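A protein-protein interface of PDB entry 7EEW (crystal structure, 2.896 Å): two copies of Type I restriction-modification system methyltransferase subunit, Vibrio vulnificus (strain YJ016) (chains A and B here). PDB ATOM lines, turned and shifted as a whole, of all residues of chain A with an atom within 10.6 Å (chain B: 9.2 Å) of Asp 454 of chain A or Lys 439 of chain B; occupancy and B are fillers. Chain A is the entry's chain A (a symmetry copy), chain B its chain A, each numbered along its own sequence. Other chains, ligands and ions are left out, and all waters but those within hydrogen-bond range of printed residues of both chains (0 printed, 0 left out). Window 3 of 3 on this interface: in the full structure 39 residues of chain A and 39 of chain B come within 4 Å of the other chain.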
ATOM      1  N   VAL A 446      27.709  -3.300 -20.244  1.00  0.00           N
ATOM      2  CA  VAL A 446      27.831  -1.924 -19.773  1.00  0.00           C
ATOM      3  C   VAL A 446      27.127  -0.941 -20.701  1.00  0.00           C
ATOM      4  O   VAL A 446      26.740   0.149 -20.257  1.00  0.00           O
ATOM      5  CB  VAL A 446      29.317  -1.549 -19.610  1.00  0.00           C
ATOM      6  CG1 VAL A 446      29.478  -0.165 -18.997  1.00  0.00           C
ATOM      7  CG2 VAL A 446      30.035  -2.588 -18.764  1.00  0.00           C
ATOM      8  N   THR A 447      26.938  -1.303 -21.974  1.00  0.00           N
ATOM      9  CA  THR A 447      26.287  -0.403 -22.923  1.00  0.00           C
ATOM     10  C   THR A 447      24.916   0.040 -22.428  1.00  0.00           C
ATOM     11  O   THR A 447      24.557   1.219 -22.541  1.00  0.00           O
ATOM     12  CB  THR A 447      26.159  -1.082 -24.289  1.00  0.00           C
ATOM     13  OG1 THR A 447      27.452  -1.184 -24.898  1.00  0.00           O
ATOM     14  CG2 THR A 447      25.231  -0.297 -25.205  1.00  0.00           C
ATOM     15  N   SER A 448      24.145  -0.880 -21.853  1.00  0.00           N
ATOM     16  CA  SER A 448      22.773  -0.580 -21.471  1.00  0.00           C
ATOM     17  C   SER A 448      22.611  -0.201 -20.005  1.00  0.00           C
ATOM     18  O   SER A 448      21.726   0.597 -19.683  1.00  0.00           O
ATOM     19  CB  SER A 448      21.866  -1.774 -21.786  1.00  0.00           C
ATOM     20  OG  SER A 448      21.920  -2.102 -23.165  1.00  0.00           O
ATOM     21  N   ILE A 449      23.441  -0.742 -19.108  1.00  0.00           N
ATOM     22  CA  ILE A 449      23.253  -0.459 -17.688  1.00  0.00           C
ATOM     23  C   ILE A 449      23.703   0.957 -17.351  1.00  0.00           C
ATOM     24  O   ILE A 449      23.127   1.605 -16.469  1.00  0.00           O
ATOM     25  CB  ILE A 449      23.980  -1.509 -16.827  1.00  0.00           C
ATOM     26  CG1 ILE A 449      25.481  -1.484 -17.104  1.00  0.00           C
ATOM     27  CG2 ILE A 449      23.412  -2.897 -17.084  1.00  0.00           C
ATOM     28  CD1 ILE A 449      26.227  -2.650 -16.513  1.00  0.00           C
ATOM     29  N   GLU A 450      24.733   1.464 -18.034  1.00  0.00           N
ATOM     30  CA  GLU A 450      25.098   2.865 -17.859  1.00  0.00           C
ATOM     31  C   GLU A 450      24.024   3.778 -18.431  1.00  0.00           C
ATOM     32  O   GLU A 450      23.737   4.840 -17.869  1.00  0.00           O
ATOM     33  CB  GLU A 450      26.452   3.145 -18.510  1.00  0.00           C
ATOM     34  CG  GLU A 450      27.644   2.758 -17.651  1.00  0.00           C
ATOM     35  CD  GLU A 450      27.786   3.642 -16.427  1.00  0.00           C
ATOM     36  OE1 GLU A 450      27.435   4.837 -16.513  1.00  0.00           O
ATOM     37  OE2 GLU A 450      28.242   3.138 -15.379  1.00  0.00           O
ATOM     38  N   ASN A 451      23.416   3.374 -19.549  1.00  0.00           N
ATOM     39  CA  ASN A 451      22.269   4.106 -20.072  1.00  0.00           C
ATOM     40  C   ASN A 451      21.069   3.966 -19.143  1.00  0.00           C
ATOM     41  O   ASN A 451      20.291   4.913 -18.974  1.00  0.00           O
ATOM     42  CB  ASN A 451      21.931   3.607 -21.477  1.00  0.00           C
ATOM     43  CG  ASN A 451      21.144   4.621 -22.284  1.00  0.00           C
ATOM     44  OD1 ASN A 451      19.946   4.806 -22.073  1.00  0.00           O
ATOM     45  ND2 ASN A 451      21.815   5.278 -23.223  1.00  0.00           N
ATOM     46  N   HIS A 452      20.912   2.793 -18.523  1.00  0.00           N
ATOM     47  CA  HIS A 452      19.831   2.589 -17.564  1.00  0.00           C
ATOM     48  C   HIS A 452      20.085   3.359 -16.273  1.00  0.00           C
ATOM     49  O   HIS A 452      19.147   3.894 -15.670  1.00  0.00           O
ATOM     50  CB  HIS A 452      19.665   1.095 -17.278  1.00  0.00           C
ATOM     51  CG  HIS A 452      18.566   0.775 -16.312  1.00  0.00           C
ATOM     52  ND1 HIS A 452      17.241   1.044 -16.575  1.00  0.00           N
ATOM     53  CD2 HIS A 452      18.597   0.199 -15.087  1.00  0.00           C
ATOM     54  CE1 HIS A 452      16.503   0.651 -15.552  1.00  0.00           C
ATOM     55  NE2 HIS A 452      17.302   0.136 -14.635  1.00  0.00           N
ATOM     56  N   PHE A 453      21.346   3.425 -15.837  1.00  0.00           N
ATOM     57  CA  PHE A 453      21.690   4.188 -14.640  1.00  0.00           C
ATOM     58  C   PHE A 453      21.300   5.654 -14.789  1.00  0.00           C
ATOM     59  O   PHE A 453      20.561   6.203 -13.965  1.00  0.00           O
ATOM     60  CB  PHE A 453      23.188   4.068 -14.354  1.00  0.00           C
ATOM     61  CG  PHE A 453      23.537   3.033 -13.324  1.00  0.00           C
ATOM     62  CD1 PHE A 453      22.676   2.751 -12.276  1.00  0.00           C
ATOM     63  CD2 PHE A 453      24.735   2.346 -13.402  1.00  0.00           C
ATOM     64  CE1 PHE A 453      23.006   1.799 -11.327  1.00  0.00           C
ATOM     65  CE2 PHE A 453      25.071   1.394 -12.459  1.00  0.00           C
ATOM     66  CZ  PHE A 453      24.206   1.120 -11.420  1.00  0.00           C
ATOM     67  N   ASP A 454      21.795   6.310 -15.841  1.00  0.00           N
ATOM     68  CA  ASP A 454      21.594   7.747 -15.963  1.00  0.00           C
ATOM     69  C   ASP A 454      20.176   8.103 -16.396  1.00  0.00           C
ATOM     70  O   ASP A 454      19.759   9.254 -16.219  1.00  0.00           O
ATOM     71  CB  ASP A 454      22.610   8.339 -16.938  1.00  0.00           C
ATOM     72  CG  ASP A 454      24.038   8.215 -16.437  1.00  0.00           C
ATOM     73  OD1 ASP A 454      24.232   7.807 -15.272  1.00  0.00           O
ATOM     74  OD2 ASP A 454      24.968   8.522 -17.211  1.00  0.00           O
ATOM     75  N   TYR A 455      19.423   7.152 -16.952  1.00  0.00           N
ATOM     76  CA  TYR A 455      18.025   7.414 -17.271  1.00  0.00           C
ATOM     77  C   TYR A 455      17.122   7.310 -16.047  1.00  0.00           C
ATOM     78  O   TYR A 455      15.990   7.802 -16.085  1.00  0.00           O
ATOM     79  CB  TYR A 455      17.545   6.458 -18.367  1.00  0.00           C
ATOM     80  CG  TYR A 455      16.156   6.764 -18.884  1.00  0.00           C
ATOM     81  CD1 TYR A 455      15.854   8.006 -19.426  1.00  0.00           C
ATOM     82  CD2 TYR A 455      15.151   5.808 -18.838  1.00  0.00           C
ATOM     83  CE1 TYR A 455      14.589   8.290 -19.899  1.00  0.00           C
ATOM     84  CE2 TYR A 455      13.883   6.081 -19.311  1.00  0.00           C
ATOM     85  CZ  TYR A 455      13.607   7.324 -19.841  1.00  0.00           C
ATOM     86  OH  TYR A 455      12.344   7.600 -20.312  1.00  0.00           O
ATOM     87  N   MET A 456      17.601   6.693 -14.965  1.00  0.00           N
ATOM     88  CA  MET A 456      16.846   6.621 -13.720  1.00  0.00           C
ATOM     89  C   MET A 456      17.014   7.858 -12.849  1.00  0.00           C
ATOM     90  O   MET A 456      16.263   8.018 -11.881  1.00  0.00           O
ATOM     91  CB  MET A 456      17.259   5.388 -12.912  1.00  0.00           C
ATOM     92  CG  MET A 456      16.692   4.080 -13.426  1.00  0.00           C
ATOM     93  SD  MET A 456      16.757   2.762 -12.193  1.00  0.00           S
ATOM     94  CE  MET A 456      18.512   2.411 -12.149  1.00  0.00           C
ATOM     95  N   SER A 457      17.972   8.730 -13.161  1.00  0.00           N
ATOM     96  CA  SER A 457      18.295   9.874 -12.321  1.00  0.00           C
ATOM     97  C   SER A 457      17.651  11.166 -12.811  1.00  0.00           C
ATOM     98  O   SER A 457      18.110  12.254 -12.448  1.00  0.00           O
ATOM     99  CB  SER A 457      19.812  10.044 -12.233  1.00  0.00           C
ATOM    100  OG  SER A 457      20.390  10.097 -13.525  1.00  0.00           O
ATOM    101  N   LEU A 458      16.595  11.070 -13.620  1.00  0.00           N
ATOM    102  CA  LEU A 458      15.999  12.271 -14.197  1.00  0.00           C
ATOM    103  C   LEU A 458      15.217  13.057 -13.151  1.00  0.00           C
ATOM    104  O   LEU A 458      15.364  14.280 -13.045  1.00  0.00           O
ATOM    105  CB  LEU A 458      15.104  11.894 -15.379  1.00  0.00           C
ATOM    106  CG  LEU A 458      15.758  11.096 -16.511  1.00  0.00           C
ATOM    107  CD1 LEU A 458      14.871  11.113 -17.745  1.00  0.00           C
ATOM    108  CD2 LEU A 458      17.151  11.625 -16.832  1.00  0.00           C
ATOM    109  N   ASN A 459      14.386  12.370 -12.368  1.00  0.00           N
ATOM    110  CA  ASN A 459      13.588  12.982 -11.306  1.00  0.00           C
ATOM    111  C   ASN A 459      12.721  14.115 -11.858  1.00  0.00           C
ATOM    112  O   ASN A 459      12.842  15.281 -11.478  1.00  0.00           O
ATOM    113  CB  ASN A 459      14.486  13.471 -10.164  1.00  0.00           C
ATOM    114  CG  ASN A 459      13.692  13.986  -8.975  1.00  0.00           C
ATOM    115  OD1 ASN A 459      13.386  13.240  -8.046  1.00  0.00           O
ATOM    116  ND2 ASN A 459      13.355  15.272  -9.001  1.00  0.00           N
ATOM    117  N   LEU A 460      11.839  13.748 -12.782  1.00  0.00           N
ATOM    118  CA  LEU A 460      10.910  14.713 -13.356  1.00  0.00           C
ATOM    119  C   LEU A 460       9.853  15.073 -12.320  1.00  0.00           C
ATOM    120  O   LEU A 460       9.151  14.193 -11.811  1.00  0.00           O
ATOM    121  CB  LEU A 460      10.258  14.150 -14.617  1.00  0.00           C
ATOM    122  CG  LEU A 460      11.142  13.648 -15.766  1.00  0.00           C
ATOM    123  CD1 LEU A 460      12.397  14.500 -15.936  1.00  0.00           C
ATOM    124  CD2 LEU A 460      11.494  12.173 -15.601  1.00  0.00           C
ATOM    125  N   TRP A 601       8.062   7.375 -18.930  1.00  0.00           N
ATOM    126  CA  TRP A 601       9.265   7.201 -18.125  1.00  0.00           C
ATOM    127  C   TRP A 601       9.201   5.907 -17.325  1.00  0.00           C
ATOM    128  O   TRP A 601      10.201   5.189 -17.215  1.00  0.00           O
ATOM    129  CB  TRP A 601       9.462   8.400 -17.195  1.00  0.00           C
ATOM    130  CG  TRP A 601      10.782   8.397 -16.474  1.00  0.00           C
ATOM    131  CD1 TRP A 601      12.002   8.720 -16.995  1.00  0.00           C
ATOM    132  CD2 TRP A 601      11.011   8.062 -15.097  1.00  0.00           C
ATOM    133  NE1 TRP A 601      12.976   8.604 -16.033  1.00  0.00           N
ATOM    134  CE2 TRP A 601      12.394   8.203 -14.859  1.00  0.00           C
ATOM    135  CE3 TRP A 601      10.184   7.659 -14.046  1.00  0.00           C
ATOM    136  CZ2 TRP A 601      12.966   7.953 -13.612  1.00  0.00           C
ATOM    137  CZ3 TRP A 601      10.754   7.410 -12.809  1.00  0.00           C
ATOM    138  CH2 TRP A 601      12.131   7.559 -12.603  1.00  0.00           C
ATOM    139  N   ILE A 605      11.966   2.525 -18.077  1.00  0.00           N
ATOM    140  CA  ILE A 605      12.855   2.005 -17.045  1.00  0.00           C
ATOM    141  C   ILE A 605      12.489   0.566 -16.695  1.00  0.00           C
ATOM    142  O   ILE A 605      13.360  -0.234 -16.330  1.00  0.00           O
ATOM    143  CB  ILE A 605      12.827   2.920 -15.803  1.00  0.00           C
ATOM    144  CG1 ILE A 605      13.686   2.347 -14.674  1.00  0.00           C
ATOM    145  CG2 ILE A 605      11.409   3.124 -15.316  1.00  0.00           C
ATOM    146  CD1 ILE A 605      13.339   2.897 -13.305  1.00  0.00           C
ATOM    147  N   SER A 608      13.909  -1.792 -19.519  1.00  0.00           N
ATOM    148  CA  SER A 608      15.349  -1.954 -19.357  1.00  0.00           C
ATOM    149  C   SER A 608      15.674  -2.884 -18.197  1.00  0.00           C
ATOM    150  O   SER A 608      16.653  -3.635 -18.262  1.00  0.00           O
ATOM    151  CB  SER A 608      16.011  -0.593 -19.152  1.00  0.00           C
ATOM    152  OG  SER A 608      17.420  -0.716 -19.084  1.00  0.00           O
ATOM    153  N   GLN B 432      18.709   8.702  -4.068  1.00  0.00           N
ATOM    154  CA  GLN B 432      19.667   8.574  -5.156  1.00  0.00           C
ATOM    155  C   GLN B 432      21.039   8.119  -4.680  1.00  0.00           C
ATOM    156  O   GLN B 432      21.973   8.071  -5.486  1.00  0.00           O
ATOM    157  CB  GLN B 432      19.785   9.898  -5.913  1.00  0.00           C
ATOM    158  CG  GLN B 432      18.555  10.227  -6.737  1.00  0.00           C
ATOM    159  CD  GLN B 432      18.196   9.115  -7.705  1.00  0.00           C
ATOM    160  OE1 GLN B 432      18.991   8.750  -8.570  1.00  0.00           O
ATOM    161  NE2 GLN B 432      16.997   8.562  -7.554  1.00  0.00           N
ATOM    162  N   GLU B 433      21.185   7.792  -3.394  1.00  0.00           N
ATOM    163  CA  GLU B 433      22.417   7.179  -2.917  1.00  0.00           C
ATOM    164  C   GLU B 433      22.503   5.710  -3.301  1.00  0.00           C
ATOM    165  O   GLU B 433      23.594   5.132  -3.253  1.00  0.00           O
ATOM    166  CB  GLU B 433      22.524   7.322  -1.399  1.00  0.00           C
ATOM    167  CG  GLU B 433      21.356   6.704  -0.647  1.00  0.00           C
ATOM    168  CD  GLU B 433      21.791   5.668   0.371  1.00  0.00           C
ATOM    169  OE1 GLU B 433      20.920   5.150   1.100  1.00  0.00           O
ATOM    170  OE2 GLU B 433      23.002   5.371   0.442  1.00  0.00           O
ATOM    171  N   MET B 434      21.379   5.098  -3.680  1.00  0.00           N
ATOM    172  CA  MET B 434      21.393   3.692  -4.069  1.00  0.00           C
ATOM    173  C   MET B 434      22.146   3.491  -5.377  1.00  0.00           C
ATOM    174  O   MET B 434      22.972   2.579  -5.493  1.00  0.00           O
ATOM    175  CB  MET B 434      19.962   3.163  -4.178  1.00  0.00           C
ATOM    176  CG  MET B 434      19.327   2.855  -2.837  1.00  0.00           C
ATOM    177  SD  MET B 434      20.404   1.817  -1.829  1.00  0.00           S
ATOM    178  CE  MET B 434      19.404   1.597  -0.361  1.00  0.00           C
ATOM    179  N   ILE B 435      21.874   4.336  -6.376  1.00  0.00           N
ATOM    180  CA  ILE B 435      22.614   4.255  -7.633  1.00  0.00           C
ATOM    181  C   ILE B 435      24.088   4.560  -7.406  1.00  0.00           C
ATOM    182  O   ILE B 435      24.959   3.988  -8.073  1.00  0.00           O
ATOM    183  CB  ILE B 435      21.980   5.190  -8.686  1.00  0.00           C
ATOM    184  CG1 ILE B 435      23.038   5.747  -9.644  1.00  0.00           C
ATOM    185  CG2 ILE B 435      21.202   6.309  -8.016  1.00  0.00           C
ATOM    186  CD1 ILE B 435      22.470   6.594 -10.761  1.00  0.00           C
ATOM    187  N   ALA B 436      24.395   5.443  -6.451  1.00  0.00           N
ATOM    188  CA  ALA B 436      25.787   5.711  -6.102  1.00  0.00           C
ATOM    189  C   ALA B 436      26.487   4.441  -5.631  1.00  0.00           C
ATOM    190  O   ALA B 436      27.607   4.139  -6.060  1.00  0.00           O
ATOM    191  CB  ALA B 436      25.857   6.799  -5.031  1.00  0.00           C
ATOM    192  N   SER B 437      25.838   3.678  -4.746  1.00  0.00           N
ATOM    193  CA  SER B 437      26.390   2.389  -4.342  1.00  0.00           C
ATOM    194  C   SER B 437      26.194   1.330  -5.418  1.00  0.00           C
ATOM    195  O   SER B 437      26.999   0.397  -5.517  1.00  0.00           O
ATOM    196  CB  SER B 437      25.758   1.928  -3.027  1.00  0.00           C
ATOM    197  OG  SER B 437      26.216   2.712  -1.938  1.00  0.00           O
ATOM    198  N   LEU B 438      25.141   1.455  -6.230  1.00  0.00           N
ATOM    199  CA  LEU B 438      24.958   0.521  -7.335  1.00  0.00           C
ATOM    200  C   LEU B 438      25.999   0.743  -8.423  1.00  0.00           C
ATOM    201  O   LEU B 438      26.395  -0.211  -9.104  1.00  0.00           O
ATOM    202  CB  LEU B 438      23.545   0.648  -7.908  1.00  0.00           C
ATOM    203  CG  LEU B 438      22.853  -0.661  -8.291  1.00  0.00           C
ATOM    204  CD1 LEU B 438      22.631  -1.524  -7.058  1.00  0.00           C
ATOM    205  CD2 LEU B 438      21.536  -0.395  -9.005  1.00  0.00           C
ATOM    206  N   LYS B 439      26.451   1.987  -8.604  1.00  0.00           N
ATOM    207  CA  LYS B 439      27.569   2.237  -9.508  1.00  0.00           C
ATOM    208  C   LYS B 439      28.858   1.630  -8.972  1.00  0.00           C
ATOM    209  O   LYS B 439      29.712   1.200  -9.757  1.00  0.00           O
ATOM    210  CB  LYS B 439      27.747   3.740  -9.735  1.00  0.00           C
ATOM    211  CG  LYS B 439      26.768   4.354 -10.725  1.00  0.00           C
ATOM    212  CD  LYS B 439      27.116   5.811 -11.000  1.00  0.00           C
ATOM    213  CE  LYS B 439      26.218   6.407 -12.071  1.00  0.00           C
ATOM    214  NZ  LYS B 439      26.593   7.814 -12.384  1.00  0.00           N
ATOM    215  N   SER B 440      29.018   1.589  -7.648  1.00  0.00           N
ATOM    216  CA  SER B 440      30.188   0.945  -7.060  1.00  0.00           C
ATOM    217  C   SER B 440      30.167  -0.558  -7.304  1.00  0.00           C
ATOM    218  O   SER B 440      31.216  -1.170  -7.537  1.00  0.00           O
ATOM    219  CB  SER B 440      30.261   1.247  -5.564  1.00  0.00           C
ATOM    220  OG  SER B 440      31.342   0.560  -4.957  1.00  0.00           O
ATOM    221  N   GLU B 441      28.982  -1.173  -7.247  1.00  0.00           N
ATOM    222  CA  GLU B 441      28.872  -2.588  -7.584  1.00  0.00           C
ATOM    223  C   GLU B 441      29.235  -2.828  -9.042  1.00  0.00           C
ATOM    224  O   GLU B 441      29.859  -3.842  -9.377  1.00  0.00           O
ATOM    225  CB  GLU B 441      27.458  -3.090  -7.291  1.00  0.00           C
ATOM    226  CG  GLU B 441      27.022  -2.903  -5.848  1.00  0.00           C
ATOM    227  CD  GLU B 441      25.582  -3.315  -5.613  1.00  0.00           C
ATOM    228  OE1 GLU B 441      25.062  -4.142  -6.391  1.00  0.00           O
ATOM    229  OE2 GLU B 441      24.968  -2.808  -4.650  1.00  0.00           O
ATOM    230  N   GLN B 442      28.852  -1.901  -9.923  1.00  0.00           N
ATOM    231  CA  GLN B 442      29.265  -1.997 -11.317  1.00  0.00           C
ATOM    232  C   GLN B 442      30.763  -1.778 -11.464  1.00  0.00           C
ATOM    233  O   GLN B 442      31.396  -2.379 -12.340  1.00  0.00           O
ATOM    234  CB  GLN B 442      28.488  -0.992 -12.166  1.00  0.00           C
ATOM    235  CG  GLN B 442      28.884  -0.982 -13.633  1.00  0.00           C
ATOM    236  CD  GLN B 442      28.721  -2.339 -14.293  1.00  0.00           C
ATOM    237  OE1 GLN B 442      27.940  -3.177 -13.841  1.00  0.00           O
ATOM    238  NE2 GLN B 442      29.456  -2.560 -15.375  1.00  0.00           N
ATOM    239  N   LEU B 443      31.346  -0.929 -10.617  1.00  0.00           N
ATOM    240  CA  LEU B 443      32.798  -0.792 -10.588  1.00  0.00           C
ATOM    241  C   LEU B 443      33.462  -2.113 -10.221  1.00  0.00           C
ATOM    242  O   LEU B 443      34.440  -2.524 -10.856  1.00  0.00           O
ATOM    243  CB  LEU B 443      33.196   0.316  -9.609  1.00  0.00           C
ATOM    244  CG  LEU B 443      34.635   0.369  -9.093  1.00  0.00           C
ATOM    245  CD1 LEU B 443      35.116   1.808  -9.021  1.00  0.00           C
ATOM    246  CD2 LEU B 443      34.742  -0.288  -7.721  1.00  0.00           C
ATOM    247  N   SER B 444      32.940  -2.797  -9.200  1.00  0.00           N
ATOM    248  CA  SER B 444      33.447  -4.118  -8.850  1.00  0.00           C
ATOM    249  C   SER B 444      33.014  -5.180  -9.853  1.00  0.00           C
ATOM    250  O   SER B 444      33.664  -6.227  -9.951  1.00  0.00           O
ATOM    251  CB  SER B 444      32.987  -4.510  -7.445  1.00  0.00           C
ATOM    252  OG  SER B 444      33.707  -3.809  -6.450  1.00  0.00           O
ATOM    253  N   LEU B 445      31.938  -4.930 -10.601  1.00  0.00           N
ATOM    254  CA  LEU B 445      31.477  -5.909 -11.581  1.00  0.00           C
ATOM    255  C   LEU B 445      32.516  -6.109 -12.677  1.00  0.00           C
ATOM    256  O   LEU B 445      32.939  -7.238 -12.952  1.00  0.00           O
ATOM    257  CB  LEU B 445      30.137  -5.463 -12.170  1.00  0.00           C
ATOM    258  CG  LEU B 445      29.165  -6.539 -12.664  1.00  0.00           C
ATOM    259  CD1 LEU B 445      29.531  -7.031 -14.055  1.00  0.00           C
ATOM    260  CD2 LEU B 445      29.111  -7.695 -11.680  1.00  0.00           C
ATOM    261  N   VAL B 446      32.962  -5.012 -13.296  1.00  0.00           N
ATOM    262  CA  VAL B 446      33.998  -5.085 -14.322  1.00  0.00           C
ATOM    263  C   VAL B 446      35.380  -5.306 -13.718  1.00  0.00           C
ATOM    264  O   VAL B 446      36.269  -5.830 -14.403  1.00  0.00           O
ATOM    265  CB  VAL B 446      33.979  -3.810 -15.187  1.00  0.00           C
ATOM    266  CG1 VAL B 446      34.960  -3.909 -16.347  1.00  0.00           C
ATOM    267  CG2 VAL B 446      32.575  -3.543 -15.704  1.00  0.00           C
ATOM    268  N   THR B 447      35.580  -4.931 -12.450  1.00  0.00           N
ATOM    269  CA  THR B 447      36.885  -5.096 -11.814  1.00  0.00           C
ATOM    270  C   THR B 447      37.367  -6.539 -11.884  1.00  0.00           C
ATOM    271  O   THR B 447      38.545  -6.797 -12.163  1.00  0.00           O
ATOM    272  CB  THR B 447      36.823  -4.631 -10.357  1.00  0.00           C
ATOM    273  OG1 THR B 447      36.708  -3.204 -10.313  1.00  0.00           O
ATOM    274  CG2 THR B 447      38.066  -5.061  -9.592  1.00  0.00           C
ATOM    275  N   PHE B 619      23.763  -8.522  -7.861  1.00  0.00           N
ATOM    276  CA  PHE B 619      23.599  -7.316  -8.664  1.00  0.00           C
ATOM    277  C   PHE B 619      22.334  -7.370  -9.512  1.00  0.00           C
ATOM    278  O   PHE B 619      21.739  -6.326  -9.798  1.00  0.00           O
ATOM    279  CB  PHE B 619      24.827  -7.111  -9.551  1.00  0.00           C
ATOM    280  CG  PHE B 619      24.804  -5.833 -10.340  1.00  0.00           C
ATOM    281  CD1 PHE B 619      25.304  -4.662  -9.796  1.00  0.00           C
ATOM    282  CD2 PHE B 619      24.292  -5.805 -11.627  1.00  0.00           C
ATOM    283  CE1 PHE B 619      25.288  -3.484 -10.519  1.00  0.00           C
ATOM    284  CE2 PHE B 619      24.272  -4.632 -12.354  1.00  0.00           C
ATOM    285  CZ  PHE B 619      24.772  -3.469 -11.800  1.00  0.00           C
ATOM    286  N   LEU B 623      19.455  -4.405  -8.835  1.00  0.00           N
ATOM    287  CA  LEU B 623      19.001  -3.474  -9.861  1.00  0.00           C
ATOM    288  C   LEU B 623      17.489  -3.535 -10.031  1.00  0.00           C
ATOM    289  O   LEU B 623      16.864  -2.528 -10.381  1.00  0.00           O
ATOM    290  CB  LEU B 623      19.702  -3.767 -11.189  1.00  0.00           C
ATOM    291  CG  LEU B 623      19.396  -2.823 -12.354  1.00  0.00           C
ATOM    292  CD1 LEU B 623      20.681  -2.396 -13.043  1.00  0.00           C
ATOM    293  CD2 LEU B 623      18.446  -3.471 -13.352  1.00  0.00           C
ATOM    294  N   ILE B 626      16.023  -1.530  -7.087  1.00  0.00           N
ATOM    295  CA  ILE B 626      16.323  -0.113  -7.261  1.00  0.00           C
ATOM    296  C   ILE B 626      15.428   0.492  -8.336  1.00  0.00           C
ATOM    297  O   ILE B 626      14.958   1.628  -8.207  1.00  0.00           O
ATOM    298  CB  ILE B 626      17.818   0.082  -7.582  1.00  0.00           C
ATOM    299  CG1 ILE B 626      18.597   0.456  -6.317  1.00  0.00           C
ATOM    300  CG2 ILE B 626      18.021   1.141  -8.661  1.00  0.00           C
ATOM    301  CD1 ILE B 626      18.567  -0.598  -5.233  1.00  0.00           C
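The side-chain amino group (NZ) of Lys 439 of chain B lies within salt-bridge range of the side-chain carboxylate (OD1) of Asp 454 of chain A, at 3.7 Å.
A ring nitrogen (NE2) of His 452 of chain A sits close to the side-chain sulfur (SD) of Met 456 of chain A. The side-chain hydroxyl (OG) of Ser 608 of chain A sits at hydrogen-bond distance from a ring nitrogen (ND1) of His 452 of chain A (3.1 Å). OG of Ser 457 of chain A lies within hydrogen-bond range of O of Asp 454 of chain A.
NE2 of Gln 442 of chain B touches CG2 of Val 446 of chain A, at 3.4 Å. Ile 449 of chain A touches Gln 442 of chain B (CD1 to OE1, 3.2 Å). His 452 of chain A touches Leu 623 of chain B. O of Phe 453 of chain A touches CD1 of Ile 435 of chain B (3.8 Å). CZ of Phe 453 of chain A touches O of Leu 438 of chain B, at 3.5 Å. Lys 439 of chain B touches Phe 453 of chain A. CG2 of Ile 626 of chain B touches CE of Met 456 of chain A, at 3.7 Å. CB of Ser 457 of chain A touches OE1 of Gln 432 of chain B, 3.97 Å away.
Asp 454 of chain A touches one residue of chain B. Of the printed residues of chain A, Lys 439 of chain B touches Phe 453 (3.7 Å) and Asp 454 (3.7 Å). Of chain B, only Gln 432 comes within 4 Å of Ser 457 of chain A. Of chain A, only Phe 453 (3.8 Å) comes within 4 Å of Ile 435 of chain B. No residue of chain A comes within 4 Å of Ala 436 of chain B. Leu 438 of chain B touches just one residue of chain A: Phe 453 (3.5 Å). No residue of chain A comes within 4 Å of Ser 440 of chain B. Leu 443 of chain B touches none of the printed residues of chain A. Printed residues of chain A within 4 Å of Gln 432 of chain B: Ser 457 (3.97 Å). Printed residues of chain A within 4 Å of Gln 442 of chain B: Val 446 (3.4 Å) and Ile 449 (3.2 Å). Of the printed residues of chain B, Val 446 of chain A touches Gln 442 (3.4 Å). Printed residues of chain B within 4 Å of Met 456 of chain A: Ile 626 (3.7 Å). Printed residues of chain A within 4 Å of Leu 623 of chain B: His 452. Asn 451 of chain A touches none of the printed residues of chain B. The nearest residue of chain B that does not touch Asp 454 of chain A is Ile 435 of chain B (5.0 Å). The nearest residue of chain A that does not touch Lys 439 of chain B is Glu 450 of chain A (4.9 Å).
Of the 19 printed residues of chain B, 7 touch a printed residue of chain A. Printed residues of chain B that touch a printed residue of chain A: Gln 432, Ile 435, Leu 438, Lys 439, Gln 442, Leu 623 and Ile 626. Hydrophobic or aromatic side chains of chain B that line the printed part of chain A: Ile 435, Leu 438, Leu 623 and Ile 626. Among the printed residues, 9 pairs touch across the chains.
Positions printed for both chains: 446 and 447. Of the 9 pairs that touch across the chains among the printed residues, none has its exchanged pair printed and touching as well.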
